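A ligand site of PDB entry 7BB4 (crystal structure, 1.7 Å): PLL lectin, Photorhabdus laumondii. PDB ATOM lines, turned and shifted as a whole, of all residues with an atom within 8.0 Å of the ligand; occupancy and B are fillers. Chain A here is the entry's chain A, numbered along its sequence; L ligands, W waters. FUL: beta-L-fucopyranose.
The backbone NH (N) of Gly 120 lies within hydrogen-bond range of an oxygen (O5) of the ligand. An oxygen (O4) of the ligand lies within hydrogen-bond range of the backbone carbonyl oxygen (O) of Gly 120, 2.7 Å away. OG of Ser 142 sits at hydrogen-bond distance from O3 of the ligand (2.8 Å). N of Ser 142 is in hydrogen-bond range of O4 of the ligand.
OD1 of Asp 143 lies within hydrogen-bond range of NE1 of Trp 147 (2.9 Å). The backbone carbonyl oxygen (O) of Val 139 sits at hydrogen-bond distance from the backbone NH (N) of Trp 147 (2.9 Å). The backbone carbonyl oxygen of Gly 120 sits at hydrogen-bond distance from the backbone NH of Ser 142 (3.5 Å). The side-chain hydroxyl (OG1) of Thr 122 lies within hydrogen-bond range of the backbone carbonyl oxygen (O) of Gly 141 (2.8 Å). The backbone NH of Ile 121 sits at hydrogen-bond distance from the backbone carbonyl oxygen of Asn 96 (2.9 Å).
Residues that only touch the ligand: Gly 119, Ile 121, Gly 141 and Trp 147. Hydrophobic or aromatic side chains within 4 Å of the ligand: Ile 121 and Trp 147. Six residues have an atom within 4 Å of the ligand: Gly 119, Gly 120, Ile 121, Gly 141, Ser 142 and Trp 147. Along chain A the residues within 4 Å of the ligand span positions 119 to 147.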
ATOM      1  N   ASN A  96     -22.779  19.790   8.678  1.00  0.00           N
ATOM      2  CA  ASN A  96     -21.465  19.456   8.129  1.00  0.00           C
ATOM      3  C   ASN A  96     -21.224  20.086   6.764  1.00  0.00           C
ATOM      4  O   ASN A  96     -20.305  19.691   6.049  1.00  0.00           O
ATOM      5  CB  ASN A  96     -21.255  17.938   8.071  1.00  0.00           C
ATOM      6  CG  ASN A  96     -20.933  17.347   9.422  1.00  0.00           C
ATOM      7  OD1 ASN A  96     -20.451  18.044  10.326  1.00  0.00           O
ATOM      8  ND2 ASN A  96     -21.224  16.063   9.594  1.00  0.00           N
ATOM      9  N   ALA A  97     -22.012  21.090   6.416  1.00  0.00           N
ATOM     10  CA  ALA A  97     -21.791  21.892   5.212  1.00  0.00           C
ATOM     11  C   ALA A  97     -21.052  23.176   5.573  1.00  0.00           C
ATOM     12  O   ALA A  97     -20.877  23.509   6.741  1.00  0.00           O
ATOM     13  CB  ALA A  97     -23.132  22.231   4.556  1.00  0.00           C
ATOM     14  N   LEU A  98     -20.642  23.897   4.545  1.00  0.00           N
ATOM     15  CA  LEU A  98     -19.941  25.160   4.738  1.00  0.00           C
ATOM     16  C   LEU A  98     -20.932  26.305   4.804  1.00  0.00           C
ATOM     17  O   LEU A  98     -21.872  26.384   3.995  1.00  0.00           O
ATOM     18  CB  LEU A  98     -18.946  25.397   3.591  1.00  0.00           C
ATOM     19  CG  LEU A  98     -18.062  26.622   3.646  1.00  0.00           C
ATOM     20  CD1 LEU A  98     -17.093  26.513   4.806  1.00  0.00           C
ATOM     21  CD2 LEU A  98     -17.313  26.728   2.313  1.00  0.00           C
ATOM     22  N   LEU A 117     -23.143  27.578   1.859  1.00  0.00           N
ATOM     23  CA  LEU A 117     -22.378  27.224   0.671  1.00  0.00           C
ATOM     24  C   LEU A 117     -22.400  25.724   0.406  1.00  0.00           C
ATOM     25  O   LEU A 117     -21.769  25.274  -0.566  1.00  0.00           O
ATOM     26  CB  LEU A 117     -20.927  27.743   0.812  1.00  0.00           C
ATOM     27  CG  LEU A 117     -20.766  29.267   0.616  1.00  0.00           C
ATOM     28  CD1 LEU A 117     -19.374  29.747   0.961  1.00  0.00           C
ATOM     29  CD2 LEU A 117     -21.160  29.703  -0.797  1.00  0.00           C
ATOM     30  N   TYR A 118     -23.102  24.941   1.227  1.00  0.00           N
ATOM     31  CA  TYR A 118     -23.322  23.521   0.980  1.00  0.00           C
ATOM     32  C   TYR A 118     -22.012  22.737   1.045  1.00  0.00           C
ATOM     33  O   TYR A 118     -21.082  23.144   1.740  1.00  0.00           O
ATOM     34  CB  TYR A 118     -24.044  23.325  -0.357  1.00  0.00           C
ATOM     35  CG  TYR A 118     -25.370  24.058  -0.327  1.00  0.00           C
ATOM     36  CD1 TYR A 118     -26.451  23.523   0.348  1.00  0.00           C
ATOM     37  CD2 TYR A 118     -25.507  25.319  -0.896  1.00  0.00           C
ATOM     38  CE1 TYR A 118     -27.645  24.209   0.416  1.00  0.00           C
ATOM     39  CE2 TYR A 118     -26.708  26.016  -0.834  1.00  0.00           C
ATOM     40  CZ  TYR A 118     -27.778  25.436  -0.171  1.00  0.00           C
ATOM     41  OH  TYR A 118     -28.978  26.106  -0.072  1.00  0.00           O
ATOM     42  N   GLY A 119     -21.940  21.581   0.383  1.00  0.00           N
ATOM     43  CA  GLY A 119     -20.781  20.721   0.474  1.00  0.00           C
ATOM     44  C   GLY A 119     -20.811  19.813   1.697  1.00  0.00           C
ATOM     45  O   GLY A 119     -21.633  19.942   2.610  1.00  0.00           O
ATOM     46  N   GLY A 120     -19.897  18.846   1.691  1.00  0.00           N
ATOM     47  CA  GLY A 120     -19.633  17.995   2.830  1.00  0.00           C
ATOM     48  C   GLY A 120     -18.212  18.213   3.285  1.00  0.00           C
ATOM     49  O   GLY A 120     -17.262  17.952   2.532  1.00  0.00           O
ATOM     50  N   ILE A 121     -18.040  18.685   4.518  1.00  0.00           N
ATOM     51  CA  ILE A 121     -16.796  19.263   5.003  1.00  0.00           C
ATOM     52  C   ILE A 121     -16.246  18.353   6.097  1.00  0.00           C
ATOM     53  O   ILE A 121     -16.964  18.034   7.042  1.00  0.00           O
ATOM     54  CB  ILE A 121     -17.019  20.684   5.551  1.00  0.00           C
ATOM     55  CG1 ILE A 121     -17.822  21.532   4.551  1.00  0.00           C
ATOM     56  CG2 ILE A 121     -15.708  21.361   5.925  1.00  0.00           C
ATOM     57  CD1 ILE A 121     -17.268  21.529   3.141  1.00  0.00           C
ATOM     58  N   THR A 122     -14.976  17.951   5.968  1.00  0.00           N
ATOM     59  CA  THR A 122     -14.365  17.119   6.995  1.00  0.00           C
ATOM     60  C   THR A 122     -13.063  17.740   7.522  1.00  0.00           C
ATOM     61  O   THR A 122     -12.243  17.020   8.094  1.00  0.00           O
ATOM     62  CB  THR A 122     -14.101  15.703   6.476  1.00  0.00           C
ATOM     63  OG1 THR A 122     -13.102  15.748   5.450  1.00  0.00           O
ATOM     64  CG2 THR A 122     -15.393  15.116   5.886  1.00  0.00           C
ATOM     65  N   VAL A 139     -11.129  23.014   1.565  1.00  0.00           N
ATOM     66  CA  VAL A 139     -11.500  22.111   2.640  1.00  0.00           C
ATOM     67  C   VAL A 139     -11.130  20.687   2.241  1.00  0.00           C
ATOM     68  O   VAL A 139     -10.996  20.359   1.072  1.00  0.00           O
ATOM     69  CB  VAL A 139     -13.012  22.147   2.950  1.00  0.00           C
ATOM     70  CG1 VAL A 139     -13.478  23.577   3.227  1.00  0.00           C
ATOM     71  CG2 VAL A 139     -13.794  21.527   1.790  1.00  0.00           C
ATOM     72  N   ARG A 140     -10.987  19.825   3.259  1.00  0.00           N
ATOM     73  CA  ARG A 140     -11.043  18.400   2.992  1.00  0.00           C
ATOM     74  C   ARG A 140     -12.508  18.008   2.865  1.00  0.00           C
ATOM     75  O   ARG A 140     -13.363  18.509   3.590  1.00  0.00           O
ATOM     76  CB  ARG A 140     -10.371  17.582   4.097  1.00  0.00           C
ATOM     77  CG  ARG A 140     -10.220  16.106   3.741  1.00  0.00           C
ATOM     78  CD  ARG A 140      -9.474  15.336   4.817  1.00  0.00           C
ATOM     79  NE  ARG A 140     -10.269  15.188   6.028  1.00  0.00           N
ATOM     80  CZ  ARG A 140      -9.901  14.469   7.092  1.00  0.00           C
ATOM     81  NH1 ARG A 140      -8.731  13.826   7.094  1.00  0.00           N
ATOM     82  NH2 ARG A 140     -10.694  14.388   8.145  1.00  0.00           N
ATOM     83  N   GLY A 141     -12.805  17.159   1.891  1.00  0.00           N
ATOM     84  CA  GLY A 141     -14.158  16.773   1.585  1.00  0.00           C
ATOM     85  C   GLY A 141     -14.508  15.396   2.146  1.00  0.00           C
ATOM     86  O   GLY A 141     -13.736  14.767   2.867  1.00  0.00           O
ATOM     87  N   SER A 142     -15.710  14.938   1.777  1.00  0.00           N
ATOM     88  CA  SER A 142     -16.238  13.678   2.324  1.00  0.00           C
ATOM     89  C   SER A 142     -15.400  12.466   1.909  1.00  0.00           C
ATOM     90  O   SER A 142     -15.453  11.433   2.578  1.00  0.00           O
ATOM     91  CB  SER A 142     -17.697  13.483   1.893  1.00  0.00           C
ATOM     92  OG  SER A 142     -17.787  13.435   0.472  1.00  0.00           O
ATOM     93  N   ASP A 143     -14.659  12.582   0.808  1.00  0.00           N
ATOM     94  CA  ASP A 143     -13.818  11.510   0.309  1.00  0.00           C
ATOM     95  C   ASP A 143     -12.359  11.737   0.668  1.00  0.00           C
ATOM     96  O   ASP A 143     -11.480  11.054   0.113  1.00  0.00           O
ATOM     97  CB  ASP A 143     -13.968  11.401  -1.212  1.00  0.00           C
ATOM     98  CG  ASP A 143     -13.609  12.696  -1.923  1.00  0.00           C
ATOM     99  OD1 ASP A 143     -13.295  13.702  -1.234  1.00  0.00           O
ATOM    100  OD2 ASP A 143     -13.632  12.708  -3.178  1.00  0.00           O
ATOM    101  N   ASN A 144     -12.078  12.680   1.572  1.00  0.00           N
ATOM    102  CA  ASN A 144     -10.763  13.027   2.070  1.00  0.00           C
ATOM    103  C   ASN A 144      -9.913  13.742   1.037  1.00  0.00           C
ATOM    104  O   ASN A 144      -8.728  14.010   1.302  1.00  0.00           O
ATOM    105  CB  ASN A 144     -10.013  11.796   2.605  1.00  0.00           C
ATOM    106  CG  ASN A 144     -10.641  11.254   3.872  1.00  0.00           C
ATOM    107  OD1 ASN A 144     -10.963  12.023   4.782  1.00  0.00           O
ATOM    108  ND2 ASN A 144     -10.820   9.943   3.937  1.00  0.00           N
ATOM    109  N   ALA A 145     -10.474  14.081  -0.112  1.00  0.00           N
ATOM    110  CA  ALA A 145      -9.732  14.876  -1.089  1.00  0.00           C
ATOM    111  C   ALA A 145      -9.797  16.370  -0.725  1.00  0.00           C
ATOM    112  O   ALA A 145     -10.562  16.797   0.144  1.00  0.00           O
ATOM    113  CB  ALA A 145     -10.271  14.652  -2.502  1.00  0.00           C
ATOM    114  N   LEU A 146      -8.949  17.150  -1.397  1.00  0.00           N
ATOM    115  CA  LEU A 146      -9.041  18.604  -1.337  1.00  0.00           C
ATOM    116  C   LEU A 146     -10.129  19.104  -2.273  1.00  0.00           C
ATOM    117  O   LEU A 146     -10.137  18.779  -3.458  1.00  0.00           O
ATOM    118  CB  LEU A 146      -7.704  19.243  -1.722  1.00  0.00           C
ATOM    119  CG  LEU A 146      -7.642  20.782  -1.694  1.00  0.00           C
ATOM    120  CD1 LEU A 146      -7.828  21.299  -0.258  1.00  0.00           C
ATOM    121  CD2 LEU A 146      -6.316  21.283  -2.279  1.00  0.00           C
ATOM    122  N   TRP A 147     -11.039  19.916  -1.750  1.00  0.00           N
ATOM    123  CA  TRP A 147     -12.100  20.522  -2.539  1.00  0.00           C
ATOM    124  C   TRP A 147     -12.031  22.029  -2.372  1.00  0.00           C
ATOM    125  O   TRP A 147     -11.557  22.528  -1.343  1.00  0.00           O
ATOM    126  CB  TRP A 147     -13.472  20.015  -2.096  1.00  0.00           C
ATOM    127  CG  TRP A 147     -13.742  18.582  -2.457  1.00  0.00           C
ATOM    128  CD1 TRP A 147     -13.214  17.474  -1.857  1.00  0.00           C
ATOM    129  CD2 TRP A 147     -14.589  18.106  -3.506  1.00  0.00           C
ATOM    130  NE1 TRP A 147     -13.694  16.336  -2.456  1.00  0.00           N
ATOM    131  CE2 TRP A 147     -14.532  16.697  -3.474  1.00  0.00           C
ATOM    132  CE3 TRP A 147     -15.401  18.741  -4.452  1.00  0.00           C
ATOM    133  CZ2 TRP A 147     -15.263  15.899  -4.377  1.00  0.00           C
ATOM    134  CZ3 TRP A 147     -16.132  17.939  -5.341  1.00  0.00           C
ATOM    135  CH2 TRP A 147     -16.043  16.541  -5.295  1.00  0.00           C
ATOM    136  N   HIS A 148     -12.500  22.766  -3.382  1.00  0.00           N
ATOM    137  CA  HIS A 148     -12.514  24.214  -3.257  1.00  0.00           C
ATOM    138  C   HIS A 148     -13.731  24.823  -3.959  1.00  0.00           C
ATOM    139  O   HIS A 148     -14.413  24.176  -4.751  1.00  0.00           O
ATOM    140  CB  HIS A 148     -11.194  24.841  -3.759  1.00  0.00           C
ATOM    141  CG  HIS A 148     -10.863  24.608  -5.204  1.00  0.00           C
ATOM    142  ND1 HIS A 148     -10.238  25.564  -5.974  1.00  0.00           N
ATOM    143  CD2 HIS A 148     -11.015  23.528  -6.002  1.00  0.00           C
ATOM    144  CE1 HIS A 148     -10.042  25.093  -7.187  1.00  0.00           C
ATOM    145  NE2 HIS A 148     -10.507  23.858  -7.242  1.00  0.00           N
ATOM    146  N   ILE A 149     -14.006  26.070  -3.589  1.00  0.00           N
ATOM    147  CA  ILE A 149     -15.148  26.834  -4.072  1.00  0.00           C
ATOM    148  C   ILE A 149     -14.716  28.293  -4.005  1.00  0.00           C
ATOM    149  O   ILE A 149     -13.883  28.659  -3.169  1.00  0.00           O
ATOM    150  CB  ILE A 149     -16.399  26.540  -3.216  1.00  0.00           C
ATOM    151  CG1 ILE A 149     -17.658  27.113  -3.874  1.00  0.00           C
ATOM    152  CG2 ILE A 149     -16.211  27.034  -1.782  1.00  0.00           C
ATOM    153  CD1 ILE A 149     -18.959  26.806  -3.109  1.00  0.00           C
ATOM    154  N   TRP A 162     -18.785  23.501  -6.121  1.00  0.00           N
ATOM    155  CA  TRP A 162     -17.672  22.767  -5.528  1.00  0.00           C
ATOM    156  C   TRP A 162     -16.917  21.978  -6.582  1.00  0.00           C
ATOM    157  O   TRP A 162     -17.509  21.387  -7.489  1.00  0.00           O
ATOM    158  CB  TRP A 162     -18.196  21.815  -4.464  1.00  0.00           C
ATOM    159  CG  TRP A 162     -18.528  22.477  -3.170  1.00  0.00           C
ATOM    160  CD1 TRP A 162     -19.794  22.827  -2.723  1.00  0.00           C
ATOM    161  CD2 TRP A 162     -17.619  22.902  -2.167  1.00  0.00           C
ATOM    162  NE1 TRP A 162     -19.699  23.412  -1.487  1.00  0.00           N
ATOM    163  CE2 TRP A 162     -18.381  23.468  -1.122  1.00  0.00           C
ATOM    164  CE3 TRP A 162     -16.225  22.834  -2.024  1.00  0.00           C
ATOM    165  CZ2 TRP A 162     -17.788  23.975   0.042  1.00  0.00           C
ATOM    166  CZ3 TRP A 162     -15.644  23.333  -0.879  1.00  0.00           C
ATOM    167  CH2 TRP A 162     -16.425  23.903   0.143  1.00  0.00           C
ATOM    168  N   LYS A 163     -15.588  21.942  -6.452  1.00  0.00           N
ATOM    169  CA  LYS A 163     -14.751  21.222  -7.402  1.00  0.00           C
ATOM    170  C   LYS A 163     -13.625  20.529  -6.661  1.00  0.00           C
ATOM    171  O   LYS A 163     -13.103  21.053  -5.671  1.00  0.00           O
ATOM    172  CB  LYS A 163     -14.178  22.163  -8.464  1.00  0.00           C
ATOM    173  CG  LYS A 163     -13.445  21.447  -9.588  1.00  0.00           C
ATOM    174  CD  LYS A 163     -13.269  22.373 -10.796  1.00  0.00           C
ATOM    175  CE  LYS A 163     -12.541  21.676 -11.929  1.00  0.00           C
ATOM    176  NZ  LYS A 163     -12.497  22.563 -13.119  1.00  0.00           N
ATOM    177  N   SER A 164     -13.238  19.351  -7.153  1.00  0.00           N
ATOM    178  CA  SER A 164     -12.260  18.539  -6.443  1.00  0.00           C
ATOM    179  C   SER A 164     -10.862  18.768  -7.005  1.00  0.00           C
ATOM    180  O   SER A 164     -10.674  18.862  -8.226  1.00  0.00           O
ATOM    181  CB  SER A 164     -12.594  17.054  -6.537  1.00  0.00           C
ATOM    182  OG  SER A 164     -11.550  16.276  -5.995  1.00  0.00           O
HETATM  183  C1  FUL L   1     -19.679  17.802  -2.123  1.00  0.00           C
HETATM  184  C2  FUL L   1     -19.250  16.344  -1.968  1.00  0.00           C
HETATM  185  O2  FUL L   1     -19.868  15.561  -3.010  1.00  0.00           O
HETATM  186  C3  FUL L   1     -17.769  16.249  -2.076  1.00  0.00           C
HETATM  187  O3  FUL L   1     -17.378  14.854  -1.883  1.00  0.00           O
HETATM  188  C4  FUL L   1     -17.047  17.123  -1.077  1.00  0.00           C
HETATM  189  O4  FUL L   1     -17.309  16.620   0.235  1.00  0.00           O
HETATM  190  C5  FUL L   1     -17.488  18.588  -1.179  1.00  0.00           C
HETATM  191  C6  FUL L   1     -16.868  19.390  -0.079  1.00  0.00           C
HETATM  192  O5  FUL L   1     -18.965  18.682  -1.138  1.00  0.00           O
HETATM  193  O1  FUL L   1     -21.016  17.968  -1.903  1.00  0.00           O
HETATM  194  O   HOH W   1     -19.995  16.860  -5.424  1.00  0.00           O
HETATM  195  O   HOH W   2     -17.999  13.301  -4.141  1.00  0.00           O
HETATM  196  O   HOH W   3     -22.542  16.768  -0.305  1.00  0.00           O
